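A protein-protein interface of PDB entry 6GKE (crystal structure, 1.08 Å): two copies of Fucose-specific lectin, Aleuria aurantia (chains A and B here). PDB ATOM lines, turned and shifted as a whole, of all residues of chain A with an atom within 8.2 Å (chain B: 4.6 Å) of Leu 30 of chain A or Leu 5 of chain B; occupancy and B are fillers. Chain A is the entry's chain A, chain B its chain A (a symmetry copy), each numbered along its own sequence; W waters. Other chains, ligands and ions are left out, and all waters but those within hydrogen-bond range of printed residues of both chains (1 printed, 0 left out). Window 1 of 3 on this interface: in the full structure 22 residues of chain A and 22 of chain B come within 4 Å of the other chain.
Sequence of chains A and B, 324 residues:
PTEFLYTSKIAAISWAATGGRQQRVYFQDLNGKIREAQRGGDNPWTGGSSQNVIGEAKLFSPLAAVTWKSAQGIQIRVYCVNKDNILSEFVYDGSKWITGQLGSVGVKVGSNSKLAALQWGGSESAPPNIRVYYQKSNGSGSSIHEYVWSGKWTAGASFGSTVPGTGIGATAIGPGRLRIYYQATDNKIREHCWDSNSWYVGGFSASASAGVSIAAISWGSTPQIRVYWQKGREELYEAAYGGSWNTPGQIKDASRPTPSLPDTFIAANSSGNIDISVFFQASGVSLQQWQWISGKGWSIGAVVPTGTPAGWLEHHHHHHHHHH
N of Leu 30 of chain B lies within hydrogen-bond range of O of Glu 3 of chain B (3.2 Å).
The backbone NH of Phe 4 of chain A lies within hydrogen-bond range of the side-chain hydroxyl of Thr 2 of chain A (3.1 Å).
N of Leu 5 of chain B is in hydrogen-bond range of O of Gln 28 of chain B (3.0 Å).
The backbone carbonyl oxygen of Glu 3 of chain A sits at hydrogen-bond distance from the backbone NH of Leu 30 of chain A (3.2 Å).
The side-chain amide oxygen (OE1) of Gln 28 of chain B sits at hydrogen-bond distance from the backbone NH (N) of Phe 60 of chain B (2.8 Å).
The side-chain hydroxyl (OG1) of Thr 2 of chain A lies within hydrogen-bond range of the side-chain hydroxyl (OG1) of Thr 306 of chain A (3.3 Å).
Phe 60 of chain B touches Pro 1 of chain A.
O of Thr 2 of chain A touches CE2 of Phe 60 of chain B, 3.6 Å away.
Leu 30 of chain B touches Leu 5 of chain A.
Tyr 6 of chain A touches Tyr 6 of chain B (CD2 to CG, 3.4 Å).
Leu 30 of chain A touches Leu 30 of chain B.
CD1 of Leu 30 of chain A touches CD1 of Leu 59 of chain B, at 3.9 Å.
Leu 30 of chain B touches Leu 59 of chain A.
Val 285 of chain A touches Tyr 6 of chain B (CG2 to CD2, 3.8 Å).
Pro 309 of chain A touches Leu 59 of chain B (CB to CB, 3.96 Å).
CG of Pro 309 of chain A touches CD2 of Phe 60 of chain B (3.95 Å).
Of chain B, only Leu 5 (3.95 Å), Leu 30 (3.7 Å) and Leu 59 (3.9 Å) come within 4 Å of Leu 30 of chain A.
Printed residues of chain A within 4 Å of Phe 60 of chain B: Pro 1, Thr 2 and Pro 309.
Of the printed residues of chain B, Pro 309 of chain A touches Leu 59 (3.96 Å) and Phe 60 (3.95 Å).
Of the printed residues of chain A, Leu 30 of chain B touches Leu 5, Leu 30 and Leu 59.
Thr 306 of chain A touches none of the printed residues of chain B.
Hydrophobic or aromatic side chains of chain A that line the printed part of chain B: Pro 1, Leu 5, Tyr 6, Leu 30, Leu 59, Val 285 and Pro 309.
Hydrophobic or aromatic side chains of chain B that line the printed part of chain A: Leu 5, Tyr 6, Leu 30, Leu 59 and Phe 60.
Leu 5 of chain A touches Leu 30 of chain B, and with the chains exchanged Leu 30 of chain A touches Leu 5 of chain B.
Tyr 6 of chain B touches its own counterpart, Tyr 6 of chain A.
Leu 30 of chain A touches its own counterpart, Leu 30 of chain B.
Leu 30 of chain A touches Leu 59 of chain B, and with the chains exchanged Leu 59 of chain A touches Leu 30 of chain B.
Positions printed for both chains: 3, 4, 5, 6, 8, 28, 29, 30, 59 and 60.
Water W1 lies within hydrogen-bond range of the side-chain amide oxygen (OD1) of Asn 31 of chain A (2.7 Å) and the backbone carbonyl oxygen (O) of Leu 30 of chain B (2.7 Å).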
ATOM      1  N   PRO A   1       3.072  30.257 -19.024  1.00  0.00           N
ATOM      2  CA  PRO A   1       4.456  29.807 -18.965  1.00  0.00           C
ATOM      3  C   PRO A   1       5.332  30.635 -19.912  1.00  0.00           C
ATOM      4  O   PRO A   1       4.817  31.409 -20.731  1.00  0.00           O
ATOM      5  CB  PRO A   1       4.421  28.331 -19.385  1.00  0.00           C
ATOM      6  CG  PRO A   1       3.198  28.224 -20.247  1.00  0.00           C
ATOM      7  CD  PRO A   1       2.248  29.278 -19.726  1.00  0.00           C
ATOM      8  N   THR A   2       6.647  30.463 -19.774  1.00  0.00           N
ATOM      9  CA  THR A   2       7.613  31.160 -20.606  1.00  0.00           C
ATOM     10  C   THR A   2       8.624  30.152 -21.150  1.00  0.00           C
ATOM     11  O   THR A   2       8.551  28.959 -20.852  1.00  0.00           O
ATOM     12  CB  THR A   2       8.338  32.276 -19.842  1.00  0.00           C
ATOM     13  OG1 THR A   2       9.346  31.658 -19.039  1.00  0.00           O
ATOM     14  CG2 THR A   2       7.411  33.123 -18.997  1.00  0.00           C
ATOM     15  N   GLU A   3       9.589  30.674 -21.913  1.00  0.00           N
ATOM     16  CA  GLU A   3      10.638  29.832 -22.474  1.00  0.00           C
ATOM     17  C   GLU A   3      11.935  29.940 -21.659  1.00  0.00           C
ATOM     18  O   GLU A   3      12.960  29.429 -22.077  1.00  0.00           O
ATOM     19  CB  GLU A   3      10.794  30.171 -23.953  1.00  0.00           C
ATOM     20  CG  GLU A   3       9.516  29.896 -24.722  1.00  0.00           C
ATOM     21  CD  GLU A   3       9.538  30.303 -26.181  1.00  0.00           C
ATOM     22  OE1 GLU A   3      10.106  31.372 -26.494  1.00  0.00           O
ATOM     23  OE2 GLU A   3       8.987  29.541 -27.000  1.00  0.00           O
ATOM     24  N   PHE A   4      11.868  30.558 -20.474  1.00  0.00           N
ATOM     25  CA  PHE A   4      13.019  30.666 -19.567  1.00  0.00           C
ATOM     26  C   PHE A   4      13.264  29.306 -18.908  1.00  0.00           C
ATOM     27  O   PHE A   4      12.404  28.805 -18.193  1.00  0.00           O
ATOM     28  CB  PHE A   4      12.703  31.738 -18.524  1.00  0.00           C
ATOM     29  CG  PHE A   4      13.806  32.233 -17.618  1.00  0.00           C
ATOM     30  CD1 PHE A   4      15.151  31.917 -17.783  1.00  0.00           C
ATOM     31  CD2 PHE A   4      13.463  33.102 -16.593  1.00  0.00           C
ATOM     32  CE1 PHE A   4      16.110  32.448 -16.931  1.00  0.00           C
ATOM     33  CE2 PHE A   4      14.422  33.621 -15.739  1.00  0.00           C
ATOM     34  CZ  PHE A   4      15.746  33.306 -15.918  1.00  0.00           C
ATOM     35  N   LEU A   5      14.445  28.724 -19.129  1.00  0.00           N
ATOM     36  CA  LEU A   5      14.774  27.444 -18.528  1.00  0.00           C
ATOM     37  C   LEU A   5      14.859  27.600 -17.006  1.00  0.00           C
ATOM     38  O   LEU A   5      15.596  28.440 -16.489  1.00  0.00           O
ATOM     39  CB  LEU A   5      16.104  26.965 -19.109  1.00  0.00           C
ATOM     40  CG  LEU A   5      16.657  25.656 -18.553  1.00  0.00           C
ATOM     41  CD1 LEU A   5      15.810  24.472 -18.996  1.00  0.00           C
ATOM     42  CD2 LEU A   5      18.108  25.495 -18.993  1.00  0.00           C
ATOM     43  N   TYR A   6      14.139  26.744 -16.281  1.00  0.00           N
ATOM     44  CA  TYR A   6      14.175  26.778 -14.822  1.00  0.00           C
ATOM     45  C   TYR A   6      15.563  26.333 -14.357  1.00  0.00           C
ATOM     46  O   TYR A   6      16.033  25.274 -14.764  1.00  0.00           O
ATOM     47  CB  TYR A   6      13.087  25.888 -14.221  1.00  0.00           C
ATOM     48  CG  TYR A   6      13.175  25.716 -12.728  1.00  0.00           C
ATOM     49  CD1 TYR A   6      13.166  26.807 -11.875  1.00  0.00           C
ATOM     50  CD2 TYR A   6      13.270  24.454 -12.170  1.00  0.00           C
ATOM     51  CE1 TYR A   6      13.238  26.650 -10.502  1.00  0.00           C
ATOM     52  CE2 TYR A   6      13.327  24.278 -10.799  1.00  0.00           C
ATOM     53  CZ  TYR A   6      13.323  25.379  -9.964  1.00  0.00           C
ATOM     54  OH  TYR A   6      13.379  25.182  -8.613  1.00  0.00           O
ATOM     55  N   SER A   8      18.178  28.039 -15.131  1.00  0.00           N
ATOM     56  CA  SER A   8      19.128  28.730 -15.996  1.00  0.00           C
ATOM     57  C   SER A   8      20.019  29.643 -15.153  1.00  0.00           C
ATOM     58  O   SER A   8      19.541  30.325 -14.248  1.00  0.00           O
ATOM     59  CB  SER A   8      18.392  29.569 -17.008  1.00  0.00           C
ATOM     60  OG  SER A   8      19.270  30.331 -17.820  1.00  0.00           O
ATOM     61  N   PHE A  27      20.133  34.777 -20.676  1.00  0.00           N
ATOM     62  CA  PHE A  27      19.561  33.632 -20.002  1.00  0.00           C
ATOM     63  C   PHE A  27      19.427  32.511 -21.028  1.00  0.00           C
ATOM     64  O   PHE A  27      19.528  32.748 -22.229  1.00  0.00           O
ATOM     65  CB  PHE A  27      18.206  33.989 -19.382  1.00  0.00           C
ATOM     66  CG  PHE A  27      17.138  34.353 -20.386  1.00  0.00           C
ATOM     67  CD1 PHE A  27      16.984  35.656 -20.842  1.00  0.00           C
ATOM     68  CD2 PHE A  27      16.289  33.380 -20.894  1.00  0.00           C
ATOM     69  CE1 PHE A  27      16.003  35.970 -21.775  1.00  0.00           C
ATOM     70  CE2 PHE A  27      15.311  33.694 -21.825  1.00  0.00           C
ATOM     71  CZ  PHE A  27      15.170  34.988 -22.262  1.00  0.00           C
ATOM     72  N   GLN A  28      19.160  31.300 -20.544  1.00  0.00           N
ATOM     73  CA  GLN A  28      19.020  30.158 -21.422  1.00  0.00           C
ATOM     74  C   GLN A  28      17.545  29.787 -21.563  1.00  0.00           C
ATOM     75  O   GLN A  28      16.769  29.858 -20.607  1.00  0.00           O
ATOM     76  CB  GLN A  28      19.833  28.981 -20.885  1.00  0.00           C
ATOM     77  CG  GLN A  28      20.027  27.859 -21.889  1.00  0.00           C
ATOM     78  CD  GLN A  28      21.114  26.914 -21.445  1.00  0.00           C
ATOM     79  OE1 GLN A  28      21.241  26.600 -20.256  1.00  0.00           O
ATOM     80  NE2 GLN A  28      21.914  26.453 -22.398  1.00  0.00           N
ATOM     81  N   ASP A  29      17.190  29.356 -22.774  1.00  0.00           N
ATOM     82  CA  ASP A  29      15.841  28.914 -23.081  1.00  0.00           C
ATOM     83  C   ASP A  29      15.767  27.380 -23.026  1.00  0.00           C
ATOM     84  O   ASP A  29      16.748  26.677 -22.770  1.00  0.00           O
ATOM     85  CB  ASP A  29      15.345  29.513 -24.400  1.00  0.00           C
ATOM     86  CG  ASP A  29      15.987  28.990 -25.675  1.00  0.00           C
ATOM     87  OD1 ASP A  29      16.540  27.872 -25.651  1.00  0.00           O
ATOM     88  OD2 ASP A  29      15.911  29.716 -26.694  1.00  0.00           O
ATOM     89  N   LEU A  30      14.558  26.859 -23.253  1.00  0.00           N
ATOM     90  CA  LEU A  30      14.294  25.419 -23.117  1.00  0.00           C
ATOM     91  C   LEU A  30      15.074  24.596 -24.147  1.00  0.00           C
ATOM     92  O   LEU A  30      15.298  23.405 -23.925  1.00  0.00           O
ATOM     93  CB  LEU A  30      12.797  25.149 -23.283  1.00  0.00           C
ATOM     94  CG  LEU A  30      11.888  25.849 -22.282  1.00  0.00           C
ATOM     95  CD1 LEU A  30      10.436  25.554 -22.605  1.00  0.00           C
ATOM     96  CD2 LEU A  30      12.213  25.436 -20.859  1.00  0.00           C
ATOM     97  N   ASN A  31      15.465  25.237 -25.254  1.00  0.00           N
ATOM     98  CA  ASN A  31      16.196  24.600 -26.341  1.00  0.00           C
ATOM     99  C   ASN A  31      17.711  24.692 -26.153  1.00  0.00           C
ATOM    100  O   ASN A  31      18.446  24.238 -27.024  1.00  0.00           O
ATOM    101  CB  ASN A  31      15.816  25.215 -27.688  1.00  0.00           C
ATOM    102  CG  ASN A  31      14.360  24.996 -28.018  1.00  0.00           C
ATOM    103  OD1 ASN A  31      13.844  23.900 -27.821  1.00  0.00           O
ATOM    104  ND2 ASN A  31      13.689  26.031 -28.492  1.00  0.00           N
ATOM    105  N   GLY A  32      18.173  25.314 -25.061  1.00  0.00           N
ATOM    106  CA  GLY A  32      19.601  25.473 -24.804  1.00  0.00           C
ATOM    107  C   GLY A  32      20.219  26.712 -25.441  1.00  0.00           C
ATOM    108  O   GLY A  32      21.424  26.937 -25.300  1.00  0.00           O
ATOM    109  N   LYS A  33      19.420  27.522 -26.144  1.00  0.00           N
ATOM    110  CA  LYS A  33      19.954  28.748 -26.722  1.00  0.00           C
ATOM    111  C   LYS A  33      20.125  29.801 -25.629  1.00  0.00           C
ATOM    112  O   LYS A  33      19.390  29.819 -24.649  1.00  0.00           O
ATOM    113  CB  LYS A  33      19.039  29.295 -27.817  1.00  0.00           C
ATOM    114  CG  LYS A  33      18.713  28.320 -28.934  1.00  0.00           C
ATOM    115  CD  LYS A  33      19.915  27.739 -29.625  1.00  0.00           C
ATOM    116  CE  LYS A  33      19.515  26.737 -30.688  1.00  0.00           C
ATOM    117  NZ  LYS A  33      20.629  25.838 -31.062  1.00  0.00           N
ATOM    118  N   ILE A  34      21.099  30.692 -25.834  1.00  0.00           N
ATOM    119  CA  ILE A  34      21.284  31.855 -24.994  1.00  0.00           C
ATOM    120  C   ILE A  34      20.549  33.013 -25.665  1.00  0.00           C
ATOM    121  O   ILE A  34      20.844  33.341 -26.813  1.00  0.00           O
ATOM    122  CB  ILE A  34      22.771  32.195 -24.778  1.00  0.00           C
ATOM    123  CG1 ILE A  34      23.575  30.997 -24.268  1.00  0.00           C
ATOM    124  CG2 ILE A  34      22.895  33.388 -23.842  1.00  0.00           C
ATOM    125  CD1 ILE A  34      25.073  31.188 -24.331  1.00  0.00           C
ATOM    126  N   ARG A  35      19.593  33.593 -24.936  1.00  0.00           N
ATOM    127  CA  ARG A  35      18.823  34.722 -25.408  1.00  0.00           C
ATOM    128  C   ARG A  35      19.241  35.998 -24.682  1.00  0.00           C
ATOM    129  O   ARG A  35      19.783  35.963 -23.578  1.00  0.00           O
ATOM    130  CB  ARG A  35      17.331  34.491 -25.168  1.00  0.00           C
ATOM    131  CG  ARG A  35      16.740  33.350 -25.976  1.00  0.00           C
ATOM    132  CD  ARG A  35      15.249  33.264 -25.742  1.00  0.00           C
ATOM    133  NE  ARG A  35      14.651  32.163 -26.470  1.00  0.00           N
ATOM    134  CZ  ARG A  35      13.348  31.947 -26.560  1.00  0.00           C
ATOM    135  NH1 ARG A  35      12.497  32.809 -26.021  1.00  0.00           N
ATOM    136  NH2 ARG A  35      12.910  30.867 -27.182  1.00  0.00           N
ATOM    137  N   LEU A  59      22.763  22.525 -21.900  1.00  0.00           N
ATOM    138  CA  LEU A  59      21.649  22.851 -21.026  1.00  0.00           C
ATOM    139  C   LEU A  59      22.194  23.065 -19.607  1.00  0.00           C
ATOM    140  O   LEU A  59      23.031  22.301 -19.138  1.00  0.00           O
ATOM    141  CB  LEU A  59      20.578  21.757 -21.065  1.00  0.00           C
ATOM    142  CG  LEU A  59      19.528  21.889 -22.171  1.00  0.00           C
ATOM    143  CD1 LEU A  59      18.635  23.101 -21.953  1.00  0.00           C
ATOM    144  CD2 LEU A  59      20.136  21.936 -23.559  1.00  0.00           C
ATOM    145  N   PHE A  60      21.703  24.118 -18.944  1.00  0.00           N
ATOM    146  CA  PHE A  60      22.098  24.504 -17.572  1.00  0.00           C
ATOM    147  C   PHE A  60      23.553  24.992 -17.537  1.00  0.00           C
ATOM    148  O   PHE A  60      24.171  25.021 -16.479  1.00  0.00           O
ATOM    149  CB  PHE A  60      21.833  23.375 -16.564  1.00  0.00           C
ATOM    150  CG  PHE A  60      20.438  22.817 -16.671  1.00  0.00           C
ATOM    151  CD1 PHE A  60      19.368  23.470 -16.084  1.00  0.00           C
ATOM    152  CD2 PHE A  60      20.184  21.660 -17.391  1.00  0.00           C
ATOM    153  CE1 PHE A  60      18.077  22.984 -16.215  1.00  0.00           C
ATOM    154  CE2 PHE A  60      18.894  21.167 -17.512  1.00  0.00           C
ATOM    155  CZ  PHE A  60      17.843  21.833 -16.926  1.00  0.00           C
ATOM    156  N   VAL A 285       7.623  30.771 -15.632  1.00  0.00           N
ATOM    157  CA  VAL A 285       8.879  31.094 -14.966  1.00  0.00           C
ATOM    158  C   VAL A 285       9.365  32.464 -15.452  1.00  0.00           C
ATOM    159  O   VAL A 285       9.524  32.672 -16.652  1.00  0.00           O
ATOM    160  CB  VAL A 285       9.918  29.990 -15.267  1.00  0.00           C
ATOM    161  CG1 VAL A 285      11.318  30.369 -14.814  1.00  0.00           C
ATOM    162  CG2 VAL A 285       9.511  28.653 -14.669  1.00  0.00           C
ATOM    163  N   THR A 306      10.677  36.748 -21.449  1.00  0.00           N
ATOM    164  CA  THR A 306      11.471  35.550 -21.717  1.00  0.00           C
ATOM    165  C   THR A 306      10.694  34.569 -22.604  1.00  0.00           C
ATOM    166  O   THR A 306      10.833  33.353 -22.470  1.00  0.00           O
ATOM    167  CB  THR A 306      11.905  34.866 -20.415  1.00  0.00           C
ATOM    168  OG1 THR A 306      10.759  34.544 -19.622  1.00  0.00           O
ATOM    169  CG2 THR A 306      12.836  35.715 -19.582  1.00  0.00           C
ATOM    170  N   THR A 308       7.113  33.221 -24.977  1.00  0.00           N
ATOM    171  CA  THR A 308       5.877  32.509 -24.707  1.00  0.00           C
ATOM    172  C   THR A 308       5.825  31.300 -25.628  1.00  0.00           C
ATOM    173  O   THR A 308       5.906  31.455 -26.843  1.00  0.00           O
ATOM    174  CB  THR A 308       4.643  33.386 -24.947  1.00  0.00           C
ATOM    175  OG1 THR A 308       4.735  34.557 -24.138  1.00  0.00           O
ATOM    176  CG2 THR A 308       3.347  32.677 -24.622  1.00  0.00           C
ATOM    177  N   PRO A 309       5.696  30.067 -25.096  1.00  0.00           N
ATOM    178  CA  PRO A 309       5.644  28.893 -25.958  1.00  0.00           C
ATOM    179  C   PRO A 309       4.377  28.885 -26.822  1.00  0.00           C
ATOM    180  O   PRO A 309       3.341  29.432 -26.442  1.00  0.00           O
ATOM    181  CB  PRO A 309       5.651  27.701 -24.994  1.00  0.00           C
ATOM    182  CG  PRO A 309       5.231  28.267 -23.654  1.00  0.00           C
ATOM    183  CD  PRO A 309       5.585  29.735 -23.669  1.00  0.00           C
ATOM    184  N   GLU B   3      16.205  16.125 -17.683  1.00  0.00           N
ATOM    185  CA  GLU B   3      15.479  16.612 -18.850  1.00  0.00           C
ATOM    186  C   GLU B   3      13.976  16.731 -18.563  1.00  0.00           C
ATOM    187  O   GLU B   3      13.200  16.969 -19.473  1.00  0.00           O
ATOM    188  CB  GLU B   3      15.825  15.725 -20.042  1.00  0.00           C
ATOM    189  CG  GLU B   3      17.307  15.777 -20.360  1.00  0.00           C
ATOM    190  CD  GLU B   3      17.766  14.844 -21.462  1.00  0.00           C
ATOM    191  OE1 GLU B   3      17.267  13.699 -21.520  1.00  0.00           O
ATOM    192  OE2 GLU B   3      18.620  15.273 -22.261  1.00  0.00           O
ATOM    193  N   PHE B   4      13.581  16.617 -17.290  1.00  0.00           N
ATOM    194  CA  PHE B   4      12.182  16.782 -16.873  1.00  0.00           C
ATOM    195  C   PHE B   4      11.820  18.269 -16.912  1.00  0.00           C
ATOM    196  O   PHE B   4      12.411  19.065 -16.191  1.00  0.00           O
ATOM    197  CB  PHE B   4      12.037  16.214 -15.461  1.00  0.00           C
ATOM    198  CG  PHE B   4      10.655  16.024 -14.880  1.00  0.00           C
ATOM    199  CD1 PHE B   4       9.478  16.156 -15.611  1.00  0.00           C
ATOM    200  CD2 PHE B   4      10.556  15.638 -13.552  1.00  0.00           C
ATOM    201  CE1 PHE B   4       8.247  15.923 -15.013  1.00  0.00           C
ATOM    202  CE2 PHE B   4       9.325  15.416 -12.957  1.00  0.00           C
ATOM    203  CZ  PHE B   4       8.172  15.544 -13.692  1.00  0.00           C
ATOM    204  N   LEU B   5      10.835  18.637 -17.735  1.00  0.00           N
ATOM    205  CA  LEU B   5      10.410  20.022 -17.823  1.00  0.00           C
ATOM    206  C   LEU B   5       9.789  20.452 -16.490  1.00  0.00           C
ATOM    207  O   LEU B   5       8.860  19.822 -15.983  1.00  0.00           O
ATOM    208  CB  LEU B   5       9.404  20.147 -18.966  1.00  0.00           C
ATOM    209  CG  LEU B   5       8.787  21.526 -19.182  1.00  0.00           C
ATOM    210  CD1 LEU B   5       9.817  22.508 -19.718  1.00  0.00           C
ATOM    211  CD2 LEU B   5       7.596  21.402 -20.125  1.00  0.00           C
ATOM    212  N   TYR B   6      10.271  21.568 -15.944  1.00  0.00           N
ATOM    213  CA  TYR B   6       9.726  22.091 -14.695  1.00  0.00           C
ATOM    214  C   TYR B   6       8.299  22.579 -14.950  1.00  0.00           C
ATOM    215  O   TYR B   6       8.077  23.367 -15.865  1.00  0.00           O
ATOM    216  CB  TYR B   6      10.598  23.218 -14.140  1.00  0.00           C
ATOM    217  CG  TYR B   6      10.008  23.940 -12.958  1.00  0.00           C
ATOM    218  CD1 TYR B   6       9.640  23.260 -11.809  1.00  0.00           C
ATOM    219  CD2 TYR B   6       9.815  25.309 -12.994  1.00  0.00           C
ATOM    220  CE1 TYR B   6       9.106  23.923 -10.718  1.00  0.00           C
ATOM    221  CE2 TYR B   6       9.296  25.990 -11.907  1.00  0.00           C
ATOM    222  CZ  TYR B   6       8.930  25.293 -10.771  1.00  0.00           C
ATOM    223  OH  TYR B   6       8.421  25.986  -9.709  1.00  0.00           O
ATOM    224  N   THR B   7       7.373  22.104 -14.116  1.00  0.00           N
ATOM    225  CA  THR B   7       5.908  22.325 -14.208  1.00  0.00           C
ATOM    226  C   THR B   7       5.291  21.538 -15.369  1.00  0.00           C
ATOM    227  O   THR B   7       4.139  21.773 -15.734  1.00  0.00           O
ATOM    228  CB  THR B   7       5.463  23.802 -14.185  1.00  0.00           C
ATOM    229  OG1 THR B   7       5.713  24.475 -15.419  1.00  0.00           O
ATOM    230  CG2 THR B   7       6.091  24.565 -13.042  1.00  0.00           C
ATOM    231  N   SER B   8       6.002  20.524 -15.873  1.00  0.00           N
ATOM    232  CA  SER B   8       5.367  19.490 -16.681  1.00  0.00           C
ATOM    233  C   SER B   8       4.175  18.906 -15.922  1.00  0.00           C
ATOM    234  O   SER B   8       4.257  18.657 -14.721  1.00  0.00           O
ATOM    235  CB  SER B   8       6.347  18.384 -16.971  1.00  0.00           C
ATOM    236  OG  SER B   8       5.754  17.309 -17.683  1.00  0.00           O
ATOM    237  N   GLN B  28       6.737  15.385 -19.607  1.00  0.00           N
ATOM    238  CA  GLN B  28       7.256  16.113 -20.746  1.00  0.00           C
ATOM    239  C   GLN B  28       8.710  16.507 -20.494  1.00  0.00           C
ATOM    240  O   GLN B  28       9.098  16.861 -19.378  1.00  0.00           O
ATOM    241  CB  GLN B  28       6.393  17.345 -21.018  1.00  0.00           C
ATOM    242  CG  GLN B  28       6.642  17.982 -22.373  1.00  0.00           C
ATOM    243  CD  GLN B  28       5.539  18.945 -22.731  1.00  0.00           C
ATOM    244  OE1 GLN B  28       5.028  19.678 -21.878  1.00  0.00           O
ATOM    245  NE2 GLN B  28       5.156  18.949 -24.002  1.00  0.00           N
ATOM    246  N   ASP B  29       9.494  16.468 -21.572  1.00  0.00           N
ATOM    247  CA  ASP B  29      10.894  16.855 -21.533  1.00  0.00           C
ATOM    248  C   ASP B  29      11.054  18.295 -22.044  1.00  0.00           C
ATOM    249  O   ASP B  29      10.098  18.971 -22.435  1.00  0.00           O
ATOM    250  CB  ASP B  29      11.775  15.835 -22.261  1.00  0.00           C
ATOM    251  CG  ASP B  29      11.656  15.786 -23.776  1.00  0.00           C
ATOM    252  OD1 ASP B  29      11.211  16.786 -24.375  1.00  0.00           O
ATOM    253  OD2 ASP B  29      12.030  14.734 -24.345  1.00  0.00           O
ATOM    254  N   LEU B  30      12.300  18.775 -22.016  1.00  0.00           N
ATOM    255  CA  LEU B  30      12.602  20.173 -22.357  1.00  0.00           C
ATOM    256  C   LEU B  30      12.291  20.484 -23.825  1.00  0.00           C
ATOM    257  O   LEU B  30      12.090  21.650 -24.166  1.00  0.00           O
ATOM    258  CB  LEU B  30      14.079  20.466 -22.081  1.00  0.00           C
ATOM    259  CG  LEU B  30      14.529  20.267 -20.640  1.00  0.00           C
ATOM    260  CD1 LEU B  30      16.020  20.520 -20.523  1.00  0.00           C
ATOM    261  CD2 LEU B  30      13.760  21.167 -19.692  1.00  0.00           C
ATOM    262  N   LEU B  59       4.471  22.698 -25.369  1.00  0.00           N
ATOM    263  CA  LEU B  59       5.183  22.811 -24.108  1.00  0.00           C
ATOM    264  C   LEU B  59       4.165  23.116 -23.002  1.00  0.00           C
ATOM    265  O   LEU B  59       3.273  23.939 -23.183  1.00  0.00           O
ATOM    266  CB  LEU B  59       6.277  23.880 -24.186  1.00  0.00           C
ATOM    267  CG  LEU B  59       7.634  23.413 -24.716  1.00  0.00           C
ATOM    268  CD1 LEU B  59       8.306  22.443 -23.757  1.00  0.00           C
ATOM    269  CD2 LEU B  59       7.546  22.797 -26.099  1.00  0.00           C
ATOM    270  N   PHE B  60       4.317  22.433 -21.861  1.00  0.00           N
ATOM    271  CA  PHE B  60       3.443  22.572 -20.677  1.00  0.00           C
ATOM    272  C   PHE B  60       2.036  22.032 -20.968  1.00  0.00           C
ATOM    273  O   PHE B  60       1.087  22.364 -20.267  1.00  0.00           O
ATOM    274  CB  PHE B  60       3.420  24.016 -20.151  1.00  0.00           C
ATOM    275  CG  PHE B  60       4.801  24.589 -19.970  1.00  0.00           C
ATOM    276  CD1 PHE B  60       5.549  24.287 -18.845  1.00  0.00           C
ATOM    277  CD2 PHE B  60       5.372  25.399 -20.939  1.00  0.00           C
ATOM    278  CE1 PHE B  60       6.836  24.778 -18.693  1.00  0.00           C
ATOM    279  CE2 PHE B  60       6.655  25.900 -20.781  1.00  0.00           C
ATOM    280  CZ  PHE B  60       7.385  25.585 -19.660  1.00  0.00           C
ATOM    281  N   GLN B 281       6.736  16.364  -8.476  1.00  0.00           N
ATOM    282  CA  GLN B 281       7.957  16.921  -9.046  1.00  0.00           C
ATOM    283  C   GLN B 281       8.689  17.731  -7.975  1.00  0.00           C
ATOM    284  O   GLN B 281       8.108  18.615  -7.345  1.00  0.00           O
ATOM    285  CB  GLN B 281       7.637  17.776 -10.272  1.00  0.00           C
ATOM    286  CG  GLN B 281       8.874  18.364 -10.939  1.00  0.00           C
ATOM    287  CD  GLN B 281       8.525  19.122 -12.197  1.00  0.00           C
ATOM    288  OE1 GLN B 281       7.778  20.098 -12.163  1.00  0.00           O
ATOM    289  NE2 GLN B 281       9.041  18.668 -13.331  1.00  0.00           N
HETATM  290  O   HOH W   1      11.678  23.188 -26.388  1.00  0.00           O
